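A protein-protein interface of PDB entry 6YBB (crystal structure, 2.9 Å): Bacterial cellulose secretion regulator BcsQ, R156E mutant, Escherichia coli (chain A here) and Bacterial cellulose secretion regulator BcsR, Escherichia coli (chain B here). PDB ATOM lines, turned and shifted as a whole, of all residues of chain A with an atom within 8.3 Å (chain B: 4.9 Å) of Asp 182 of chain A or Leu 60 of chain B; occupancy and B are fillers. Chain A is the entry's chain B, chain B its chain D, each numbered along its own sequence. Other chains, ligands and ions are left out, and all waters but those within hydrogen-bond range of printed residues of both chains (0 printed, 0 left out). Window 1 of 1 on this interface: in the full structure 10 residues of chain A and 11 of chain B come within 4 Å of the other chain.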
ATOM      1  N   VAL A 149     -31.258 -23.241   7.381  1.00  0.00           N
ATOM      2  CA  VAL A 149     -30.223 -23.485   6.381  1.00  0.00           C
ATOM      3  C   VAL A 149     -29.463 -22.197   6.102  1.00  0.00           C
ATOM      4  O   VAL A 149     -29.818 -21.439   5.192  1.00  0.00           O
ATOM      5  CB  VAL A 149     -30.818 -24.060   5.085  1.00  0.00           C
ATOM      6  CG1 VAL A 149     -29.732 -24.752   4.271  1.00  0.00           C
ATOM      7  CG2 VAL A 149     -31.954 -25.010   5.401  1.00  0.00           C
ATOM      8  N   ASP A 150     -28.416 -21.939   6.879  1.00  0.00           N
ATOM      9  CA  ASP A 150     -27.565 -20.778   6.674  1.00  0.00           C
ATOM     10  C   ASP A 150     -26.145 -21.133   7.098  1.00  0.00           C
ATOM     11  O   ASP A 150     -25.884 -22.220   7.621  1.00  0.00           O
ATOM     12  CB  ASP A 150     -28.099 -19.555   7.430  1.00  0.00           C
ATOM     13  CG  ASP A 150     -28.299 -19.816   8.914  1.00  0.00           C
ATOM     14  OD1 ASP A 150     -27.864 -20.876   9.413  1.00  0.00           O
ATOM     15  OD2 ASP A 150     -28.898 -18.951   9.585  1.00  0.00           O
ATOM     16  N   ALA A 151     -25.221 -20.199   6.865  1.00  0.00           N
ATOM     17  CA  ALA A 151     -23.827 -20.438   7.221  1.00  0.00           C
ATOM     18  C   ALA A 151     -23.633 -20.492   8.731  1.00  0.00           C
ATOM     19  O   ALA A 151     -22.702 -21.151   9.207  1.00  0.00           O
ATOM     20  CB  ALA A 151     -22.936 -19.361   6.606  1.00  0.00           C
ATOM     21  N   HIS A 154     -24.543 -24.015   9.811  1.00  0.00           N
ATOM     22  CA  HIS A 154     -23.559 -24.928   9.241  1.00  0.00           C
ATOM     23  C   HIS A 154     -22.282 -24.949  10.073  1.00  0.00           C
ATOM     24  O   HIS A 154     -21.650 -26.000  10.227  1.00  0.00           O
ATOM     25  CB  HIS A 154     -23.255 -24.535   7.796  1.00  0.00           C
ATOM     26  CG  HIS A 154     -22.192 -25.369   7.152  1.00  0.00           C
ATOM     27  ND1 HIS A 154     -22.451 -26.603   6.595  1.00  0.00           N
ATOM     28  CD2 HIS A 154     -20.869 -25.145   6.974  1.00  0.00           C
ATOM     29  CE1 HIS A 154     -21.331 -27.102   6.101  1.00  0.00           C
ATOM     30  NE2 HIS A 154     -20.357 -26.237   6.319  1.00  0.00           N
ATOM     31  N   ILE A 155     -21.887 -23.798  10.620  1.00  0.00           N
ATOM     32  CA  ILE A 155     -20.720 -23.756  11.495  1.00  0.00           C
ATOM     33  C   ILE A 155     -21.018 -24.467  12.806  1.00  0.00           C
ATOM     34  O   ILE A 155     -20.239 -25.308  13.269  1.00  0.00           O
ATOM     35  CB  ILE A 155     -20.278 -22.303  11.746  1.00  0.00           C
ATOM     36  CG1 ILE A 155     -19.861 -21.628  10.441  1.00  0.00           C
ATOM     37  CG2 ILE A 155     -19.137 -22.276  12.751  1.00  0.00           C
ATOM     38  CD1 ILE A 155     -18.625 -22.220   9.831  1.00  0.00           C
ATOM     39  N   HIS A 158     -20.934 -28.225  13.248  1.00  0.00           N
ATOM     40  CA  HIS A 158     -19.611 -28.825  13.350  1.00  0.00           C
ATOM     41  C   HIS A 158     -18.940 -28.560  14.692  1.00  0.00           C
ATOM     42  O   HIS A 158     -18.227 -29.430  15.201  1.00  0.00           O
ATOM     43  CB  HIS A 158     -18.711 -28.314  12.218  1.00  0.00           C
ATOM     44  CG  HIS A 158     -19.143 -28.754  10.851  1.00  0.00           C
ATOM     45  ND1 HIS A 158     -20.329 -28.350  10.276  1.00  0.00           N
ATOM     46  CD2 HIS A 158     -18.543 -29.562   9.944  1.00  0.00           C
ATOM     47  CE1 HIS A 158     -20.442 -28.890   9.075  1.00  0.00           C
ATOM     48  NE2 HIS A 158     -19.371 -29.630   8.850  1.00  0.00           N
ATOM     49  N   SER A 177     -32.502 -19.268  -3.355  1.00  0.00           N
ATOM     50  CA  SER A 177     -31.312 -18.693  -2.739  1.00  0.00           C
ATOM     51  C   SER A 177     -30.139 -19.616  -3.017  1.00  0.00           C
ATOM     52  O   SER A 177     -30.167 -20.786  -2.627  1.00  0.00           O
ATOM     53  CB  SER A 177     -31.495 -18.502  -1.233  1.00  0.00           C
ATOM     54  OG  SER A 177     -30.274 -18.124  -0.622  1.00  0.00           O
ATOM     55  N   GLN A 178     -29.111 -19.087  -3.681  1.00  0.00           N
ATOM     56  CA  GLN A 178     -27.999 -19.925  -4.112  1.00  0.00           C
ATOM     57  C   GLN A 178     -27.250 -20.504  -2.920  1.00  0.00           C
ATOM     58  O   GLN A 178     -26.983 -21.710  -2.866  1.00  0.00           O
ATOM     59  CB  GLN A 178     -27.051 -19.126  -5.005  1.00  0.00           C
ATOM     60  CG  GLN A 178     -25.977 -19.972  -5.652  1.00  0.00           C
ATOM     61  CD  GLN A 178     -26.558 -21.064  -6.521  1.00  0.00           C
ATOM     62  OE1 GLN A 178     -26.121 -22.214  -6.473  1.00  0.00           O
ATOM     63  NE2 GLN A 178     -27.553 -20.711  -7.328  1.00  0.00           N
ATOM     64  N   VAL A 179     -26.908 -19.658  -1.947  1.00  0.00           N
ATOM     65  CA  VAL A 179     -26.126 -20.138  -0.814  1.00  0.00           C
ATOM     66  C   VAL A 179     -26.931 -21.138   0.009  1.00  0.00           C
ATOM     67  O   VAL A 179     -26.391 -22.148   0.475  1.00  0.00           O
ATOM     68  CB  VAL A 179     -25.621 -18.956   0.037  1.00  0.00           C
ATOM     69  CG1 VAL A 179     -26.779 -18.173   0.648  1.00  0.00           C
ATOM     70  CG2 VAL A 179     -24.665 -19.447   1.102  1.00  0.00           C
ATOM     71  N   GLN A 180     -28.237 -20.901   0.176  1.00  0.00           N
ATOM     72  CA  GLN A 180     -29.043 -21.843   0.944  1.00  0.00           C
ATOM     73  C   GLN A 180     -29.127 -23.189   0.238  1.00  0.00           C
ATOM     74  O   GLN A 180     -29.013 -24.243   0.876  1.00  0.00           O
ATOM     75  CB  GLN A 180     -30.444 -21.286   1.198  1.00  0.00           C
ATOM     76  CG  GLN A 180     -31.375 -22.294   1.881  1.00  0.00           C
ATOM     77  CD  GLN A 180     -32.727 -21.714   2.249  1.00  0.00           C
ATOM     78  OE1 GLN A 180     -33.051 -20.585   1.889  1.00  0.00           O
ATOM     79  NE2 GLN A 180     -33.523 -22.487   2.976  1.00  0.00           N
ATOM     80  N   ASP A 181     -29.313 -23.177  -1.084  1.00  0.00           N
ATOM     81  CA  ASP A 181     -29.383 -24.433  -1.821  1.00  0.00           C
ATOM     82  C   ASP A 181     -28.045 -25.161  -1.811  1.00  0.00           C
ATOM     83  O   ASP A 181     -28.015 -26.396  -1.829  1.00  0.00           O
ATOM     84  CB  ASP A 181     -29.848 -24.178  -3.252  1.00  0.00           C
ATOM     85  CG  ASP A 181     -31.223 -23.541  -3.313  1.00  0.00           C
ATOM     86  OD1 ASP A 181     -32.011 -23.723  -2.358  1.00  0.00           O
ATOM     87  OD2 ASP A 181     -31.513 -22.854  -4.316  1.00  0.00           O
ATOM     88  N   ASP A 182     -26.935 -24.418  -1.774  1.00  0.00           N
ATOM     89  CA  ASP A 182     -25.624 -25.056  -1.707  1.00  0.00           C
ATOM     90  C   ASP A 182     -25.380 -25.668  -0.334  1.00  0.00           C
ATOM     91  O   ASP A 182     -24.845 -26.778  -0.230  1.00  0.00           O
ATOM     92  CB  ASP A 182     -24.527 -24.048  -2.047  1.00  0.00           C
ATOM     93  CG  ASP A 182     -24.547 -23.637  -3.503  1.00  0.00           C
ATOM     94  OD1 ASP A 182     -25.140 -24.376  -4.317  1.00  0.00           O
ATOM     95  OD2 ASP A 182     -23.966 -22.582  -3.835  1.00  0.00           O
ATOM     96  N   ILE A 183     -25.760 -24.958   0.731  1.00  0.00           N
ATOM     97  CA  ILE A 183     -25.626 -25.510   2.075  1.00  0.00           C
ATOM     98  C   ILE A 183     -26.549 -26.711   2.246  1.00  0.00           C
ATOM     99  O   ILE A 183     -26.190 -27.704   2.891  1.00  0.00           O
ATOM    100  CB  ILE A 183     -25.908 -24.423   3.129  1.00  0.00           C
ATOM    101  CG1 ILE A 183     -24.916 -23.264   2.988  1.00  0.00           C
ATOM    102  CG2 ILE A 183     -25.833 -25.008   4.523  1.00  0.00           C
ATOM    103  CD1 ILE A 183     -25.267 -22.047   3.827  1.00  0.00           C
ATOM    104  N   TYR A 184     -27.746 -26.642   1.658  1.00  0.00           N
ATOM    105  CA  TYR A 184     -28.688 -27.755   1.729  1.00  0.00           C
ATOM    106  C   TYR A 184     -28.131 -28.992   1.033  1.00  0.00           C
ATOM    107  O   TYR A 184     -28.103 -30.084   1.611  1.00  0.00           O
ATOM    108  CB  TYR A 184     -30.024 -27.339   1.109  1.00  0.00           C
ATOM    109  CG  TYR A 184     -31.121 -28.376   1.210  1.00  0.00           C
ATOM    110  CD1 TYR A 184     -31.214 -29.215   2.310  1.00  0.00           C
ATOM    111  CD2 TYR A 184     -32.061 -28.519   0.199  1.00  0.00           C
ATOM    112  CE1 TYR A 184     -32.218 -30.166   2.401  1.00  0.00           C
ATOM    113  CE2 TYR A 184     -33.065 -29.465   0.281  1.00  0.00           C
ATOM    114  CZ  TYR A 184     -33.140 -30.287   1.384  1.00  0.00           C
ATOM    115  OH  TYR A 184     -34.138 -31.230   1.470  1.00  0.00           O
ATOM    116  N   GLN A 185     -27.675 -28.838  -0.213  1.00  0.00           N
ATOM    117  CA  GLN A 185     -27.132 -29.969  -0.957  1.00  0.00           C
ATOM    118  C   GLN A 185     -25.879 -30.540  -0.311  1.00  0.00           C
ATOM    119  O   GLN A 185     -25.563 -31.715  -0.528  1.00  0.00           O
ATOM    120  CB  GLN A 185     -26.838 -29.556  -2.399  1.00  0.00           C
ATOM    121  CG  GLN A 185     -28.084 -29.328  -3.238  1.00  0.00           C
ATOM    122  CD  GLN A 185     -28.757 -30.625  -3.642  1.00  0.00           C
ATOM    123  OE1 GLN A 185     -28.094 -31.645  -3.840  1.00  0.00           O
ATOM    124  NE2 GLN A 185     -30.080 -30.595  -3.765  1.00  0.00           N
ATOM    125  N   LEU A 186     -25.154 -29.741   0.472  1.00  0.00           N
ATOM    126  CA  LEU A 186     -24.052 -30.291   1.252  1.00  0.00           C
ATOM    127  C   LEU A 186     -24.574 -31.054   2.465  1.00  0.00           C
ATOM    128  O   LEU A 186     -23.996 -32.072   2.860  1.00  0.00           O
ATOM    129  CB  LEU A 186     -23.099 -29.171   1.677  1.00  0.00           C
ATOM    130  CG  LEU A 186     -21.677 -29.527   2.126  1.00  0.00           C
ATOM    131  CD1 LEU A 186     -20.755 -28.346   1.889  1.00  0.00           C
ATOM    132  CD2 LEU A 186     -21.625 -29.935   3.591  1.00  0.00           C
ATOM    133  N   TRP A 187     -25.674 -30.582   3.058  1.00  0.00           N
ATOM    134  CA  TRP A 187     -26.274 -31.297   4.178  1.00  0.00           C
ATOM    135  C   TRP A 187     -26.904 -32.613   3.740  1.00  0.00           C
ATOM    136  O   TRP A 187     -26.927 -33.572   4.519  1.00  0.00           O
ATOM    137  CB  TRP A 187     -27.321 -30.422   4.863  1.00  0.00           C
ATOM    138  CG  TRP A 187     -26.741 -29.335   5.704  1.00  0.00           C
ATOM    139  CD1 TRP A 187     -25.420 -29.049   5.874  1.00  0.00           C
ATOM    140  CD2 TRP A 187     -27.463 -28.388   6.499  1.00  0.00           C
ATOM    141  NE1 TRP A 187     -25.273 -27.979   6.722  1.00  0.00           N
ATOM    142  CE2 TRP A 187     -26.514 -27.555   7.121  1.00  0.00           C
ATOM    143  CE3 TRP A 187     -28.821 -28.162   6.744  1.00  0.00           C
ATOM    144  CZ2 TRP A 187     -26.878 -26.513   7.971  1.00  0.00           C
ATOM    145  CZ3 TRP A 187     -29.181 -27.128   7.588  1.00  0.00           C
ATOM    146  CH2 TRP A 187     -28.213 -26.316   8.192  1.00  0.00           C
ATOM    147  N   LEU A 188     -27.419 -32.680   2.509  1.00  0.00           N
ATOM    148  CA  LEU A 188     -28.089 -33.893   2.051  1.00  0.00           C
ATOM    149  C   LEU A 188     -27.138 -35.075   1.945  1.00  0.00           C
ATOM    150  O   LEU A 188     -27.586 -36.225   2.010  1.00  0.00           O
ATOM    151  CB  LEU A 188     -28.759 -33.658   0.697  1.00  0.00           C
ATOM    152  CG  LEU A 188     -30.056 -32.850   0.709  1.00  0.00           C
ATOM    153  CD1 LEU A 188     -30.589 -32.644  -0.702  1.00  0.00           C
ATOM    154  CD2 LEU A 188     -31.088 -33.548   1.573  1.00  0.00           C
ATOM    155  N   SER A 190     -24.001 -35.014   3.810  1.00  0.00           N
ATOM    156  CA  SER A 190     -23.110 -34.990   4.962  1.00  0.00           C
ATOM    157  C   SER A 190     -23.814 -35.162   6.299  1.00  0.00           C
ATOM    158  O   SER A 190     -23.169 -35.594   7.262  1.00  0.00           O
ATOM    159  CB  SER A 190     -22.309 -33.677   5.000  1.00  0.00           C
ATOM    160  OG  SER A 190     -23.160 -32.555   5.174  1.00  0.00           O
ATOM    161  N   ALA B  53     -20.560 -26.112  -5.657  1.00  0.00           N
ATOM    162  CA  ALA B  53     -20.882 -25.411  -4.418  1.00  0.00           C
ATOM    163  C   ALA B  53     -19.660 -25.284  -3.518  1.00  0.00           C
ATOM    164  O   ALA B  53     -19.498 -24.279  -2.818  1.00  0.00           O
ATOM    165  CB  ALA B  53     -22.012 -26.131  -3.683  1.00  0.00           C
ATOM    166  N   LEU B  54     -18.794 -26.299  -3.512  1.00  0.00           N
ATOM    167  CA  LEU B  54     -17.574 -26.216  -2.717  1.00  0.00           C
ATOM    168  C   LEU B  54     -16.587 -25.225  -3.323  1.00  0.00           C
ATOM    169  O   LEU B  54     -15.891 -24.510  -2.595  1.00  0.00           O
ATOM    170  CB  LEU B  54     -16.940 -27.600  -2.585  1.00  0.00           C
ATOM    171  CG  LEU B  54     -17.695 -28.596  -1.706  1.00  0.00           C
ATOM    172  CD1 LEU B  54     -17.092 -29.979  -1.847  1.00  0.00           C
ATOM    173  CD2 LEU B  54     -17.672 -28.147  -0.255  1.00  0.00           C
ATOM    174  N   ARG B  56     -17.430 -22.582  -4.812  1.00  0.00           N
ATOM    175  CA  ARG B  56     -18.038 -21.260  -4.744  1.00  0.00           C
ATOM    176  C   ARG B  56     -17.874 -20.609  -3.378  1.00  0.00           C
ATOM    177  O   ARG B  56     -17.668 -19.394  -3.293  1.00  0.00           O
ATOM    178  CB  ARG B  56     -19.524 -21.366  -5.094  1.00  0.00           C
ATOM    179  CG  ARG B  56     -20.184 -20.075  -5.530  1.00  0.00           C
ATOM    180  CD  ARG B  56     -21.585 -20.381  -6.026  1.00  0.00           C
ATOM    181  NE  ARG B  56     -21.584 -21.529  -6.931  1.00  0.00           N
ATOM    182  CZ  ARG B  56     -22.581 -22.402  -7.035  1.00  0.00           C
ATOM    183  NH1 ARG B  56     -22.495 -23.417  -7.884  1.00  0.00           N
ATOM    184  NH2 ARG B  56     -23.662 -22.267  -6.281  1.00  0.00           N
ATOM    185  N   TRP B  57     -17.957 -21.394  -2.306  1.00  0.00           N
ATOM    186  CA  TRP B  57     -17.952 -20.869  -0.947  1.00  0.00           C
ATOM    187  C   TRP B  57     -16.769 -21.427  -0.170  1.00  0.00           C
ATOM    188  O   TRP B  57     -16.689 -22.651   0.034  1.00  0.00           O
ATOM    189  CB  TRP B  57     -19.263 -21.209  -0.241  1.00  0.00           C
ATOM    190  CG  TRP B  57     -20.456 -20.840  -1.051  1.00  0.00           C
ATOM    191  CD1 TRP B  57     -21.346 -21.692  -1.637  1.00  0.00           C
ATOM    192  CD2 TRP B  57     -20.882 -19.518  -1.389  1.00  0.00           C
ATOM    193  NE1 TRP B  57     -22.309 -20.979  -2.310  1.00  0.00           N
ATOM    194  CE2 TRP B  57     -22.045 -19.642  -2.173  1.00  0.00           C
ATOM    195  CE3 TRP B  57     -20.398 -18.240  -1.097  1.00  0.00           C
ATOM    196  CZ2 TRP B  57     -22.729 -18.538  -2.671  1.00  0.00           C
ATOM    197  CZ3 TRP B  57     -21.077 -17.145  -1.592  1.00  0.00           C
ATOM    198  CH2 TRP B  57     -22.229 -17.300  -2.370  1.00  0.00           C
ATOM    199  N   PRO B  58     -15.837 -20.584   0.278  1.00  0.00           N
ATOM    200  CA  PRO B  58     -14.710 -21.093   1.077  1.00  0.00           C
ATOM    201  C   PRO B  58     -15.138 -21.725   2.386  1.00  0.00           C
ATOM    202  O   PRO B  58     -14.445 -22.620   2.887  1.00  0.00           O
ATOM    203  CB  PRO B  58     -13.858 -19.839   1.316  1.00  0.00           C
ATOM    204  CG  PRO B  58     -14.264 -18.886   0.233  1.00  0.00           C
ATOM    205  CD  PRO B  58     -15.714 -19.146  -0.007  1.00  0.00           C
ATOM    206  N   LEU B  59     -16.259 -21.283   2.960  1.00  0.00           N
ATOM    207  CA  LEU B  59     -16.711 -21.840   4.229  1.00  0.00           C
ATOM    208  C   LEU B  59     -17.153 -23.288   4.072  1.00  0.00           C
ATOM    209  O   LEU B  59     -16.926 -24.111   4.965  1.00  0.00           O
ATOM    210  CB  LEU B  59     -17.850 -20.998   4.799  1.00  0.00           C
ATOM    211  CG  LEU B  59     -18.093 -21.180   6.294  1.00  0.00           C
ATOM    212  CD1 LEU B  59     -16.847 -20.761   7.065  1.00  0.00           C
ATOM    213  CD2 LEU B  59     -19.308 -20.384   6.739  1.00  0.00           C
ATOM    214  N   LEU B  60     -17.790 -23.618   2.947  1.00  0.00           N
ATOM    215  CA  LEU B  60     -18.180 -25.004   2.719  1.00  0.00           C
ATOM    216  C   LEU B  60     -16.960 -25.879   2.465  1.00  0.00           C
ATOM    217  O   LEU B  60     -16.872 -26.998   2.982  1.00  0.00           O
ATOM    218  CB  LEU B  60     -19.164 -25.095   1.552  1.00  0.00           C
ATOM    219  CG  LEU B  60     -20.492 -24.349   1.700  1.00  0.00           C
ATOM    220  CD1 LEU B  60     -21.483 -24.798   0.638  1.00  0.00           C
ATOM    221  CD2 LEU B  60     -21.075 -24.539   3.087  1.00  0.00           C
ATOM    222  N   ALA B  61     -16.001 -25.380   1.681  1.00  0.00           N
ATOM    223  CA  ALA B  61     -14.810 -26.160   1.366  1.00  0.00           C
ATOM    224  C   ALA B  61     -13.926 -26.387   2.584  1.00  0.00           C
ATOM    225  O   ALA B  61     -13.134 -27.335   2.590  1.00  0.00           O
ATOM    226  CB  ALA B  61     -14.006 -25.471   0.265  1.00  0.00           C
ATOM    227  N   GLU B  62     -14.047 -25.543   3.612  1.00  0.00           N
ATOM    228  CA  GLU B  62     -13.196 -25.678   4.788  1.00  0.00           C
ATOM    229  C   GLU B  62     -13.536 -26.926   5.592  1.00  0.00           C
ATOM    230  O   GLU B  62     -12.667 -27.477   6.276  1.00  0.00           O
ATOM    231  CB  GLU B  62     -13.316 -24.425   5.657  1.00  0.00           C
ATOM    232  CG  GLU B  62     -12.249 -24.296   6.728  1.00  0.00           C
ATOM    233  CD  GLU B  62     -12.335 -22.983   7.480  1.00  0.00           C
ATOM    234  OE1 GLU B  62     -13.238 -22.176   7.171  1.00  0.00           O
ATOM    235  OE2 GLU B  62     -11.498 -22.760   8.379  1.00  0.00           O
ATOM    236  N   PHE B  63     -14.783 -27.392   5.519  1.00  0.00           N
ATOM    237  CA  PHE B  63     -15.209 -28.589   6.231  1.00  0.00           C
ATOM    238  C   PHE B  63     -15.225 -29.826   5.341  1.00  0.00           C
ATOM    239  O   PHE B  63     -15.882 -30.817   5.679  1.00  0.00           O
ATOM    240  CB  PHE B  63     -16.586 -28.369   6.857  1.00  0.00           C
ATOM    241  CG  PHE B  63     -16.597 -27.323   7.933  1.00  0.00           C
ATOM    242  CD1 PHE B  63     -16.012 -27.572   9.164  1.00  0.00           C
ATOM    243  CD2 PHE B  63     -17.194 -26.095   7.718  1.00  0.00           C
ATOM    244  CE1 PHE B  63     -16.022 -26.612  10.159  1.00  0.00           C
ATOM    245  CE2 PHE B  63     -17.205 -25.135   8.706  1.00  0.00           C
ATOM    246  CZ  PHE B  63     -16.620 -25.392   9.930  1.00  0.00           C
ATOM    247  N   ALA B  64     -14.519 -29.792   4.216  1.00  0.00           N
ATOM    248  CA  ALA B  64     -14.442 -30.948   3.330  1.00  0.00           C
ATOM    249  C   ALA B  64     -13.144 -31.718   3.554  1.00  0.00           C
ATOM    250  O   ALA B  64     -13.035 -32.512   4.489  1.00  0.00           O
ATOM    251  CB  ALA B  64     -14.559 -30.513   1.877  1.00  0.00           C
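Ala 151 of chain A touches Leu 59 of chain B (CB to CD2, 3.8 Å). His 154 of chain A touches Leu 60 of chain B (NE2 to CD2, 3.7 Å). NE2 of His 154 of chain A touches CD2 of Phe 63 of chain B, at 3.5 Å. Leu 59 of chain B touches Ile 155 of chain A (CD1 to CD1, 3.6 Å). Ile 155 of chain A touches Phe 63 of chain B (CD1 to CE2, 3.4 Å). His 158 of chain A touches Phe 63 of chain B. CZ2 of Trp 57 of chain B touches CB of Val 179 of chain A, at 3.98 Å. Ala 53 of chain B touches Asp 182 of chain A (CB to CG, 3.6 Å). Leu 60 of chain B touches Asp 182 of chain A. Leu 186 of chain A touches Leu 54 of chain B (CD1 to CD2, 3.8 Å).
Of the 19 printed residues of chain A, 8 touch a printed residue of chain B. Hydrophobic or aromatic side chains of chain A within 4 Å of the printed part of chain B: Ala 151, His 154, Ile 155, His 158, Val 179 and Leu 186. Along chain A the printed residues that touch a printed residue of chain B span positions 151 to 186. Among the printed residues, 14 pairs touch across the chains.
Of the printed residues of chain B, Asp 182 of chain A touches Ala 53, Arg 56, Trp 57 and Leu 60. Of the printed residues of chain A, Leu 60 of chain B touches His 154 (3.7 Å), Asp 182 (3.997 Å) and Leu 186 (3.6 Å). Ala 61 of chain B touches none of the printed residues of chain A. Of the printed residues of chain A, Leu 59 of chain B touches Ala 151 and Ile 155. Printed residues of chain B within 4 Å of Ile 155 of chain A: Leu 59 (3.6 Å) and Phe 63 (3.4 Å). The nearest printed residue of chain B that does not touch Asp 182 of chain A is Leu 54 of chain B (6.3 Å). The nearest printed residue of chain B that does not touch Val 179 of chain A is Leu 60 of chain B (5.6 Å).
The side-chain amide oxygen (OE1) of Gln 178 of chain A is in hydrogen-bond range of the guanidinium group (NH2) of Arg 56 of chain B. The side-chain carboxylate (OD2) of Asp 182 of chain A is in salt-bridge range of the guanidinium group (NH2) of Arg 56 of chain B, at 2.5 Å. The side-chain carboxylate (OD2) of Asp 182 of chain A is in hydrogen-bond range of the indole nitrogen (NE1) of Trp 57 of chain B, at 2.8 Å.
The backbone carbonyl oxygen (O) of His 154 of chain A is in hydrogen-bond range of a ring nitrogen (ND1) of His 158 of chain A, at 2.7 Å. ND1 of His 154 of chain A sits at hydrogen-bond distance from NE1 of Trp 187 of chain A (3.1 Å). OE1 of Gln 178 of chain A lies close to OD1 of Asp 182 of chain A. OG of Ser 190 of chain A lies within hydrogen-bond range of O of Leu 186 of chain A (2.5 Å).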
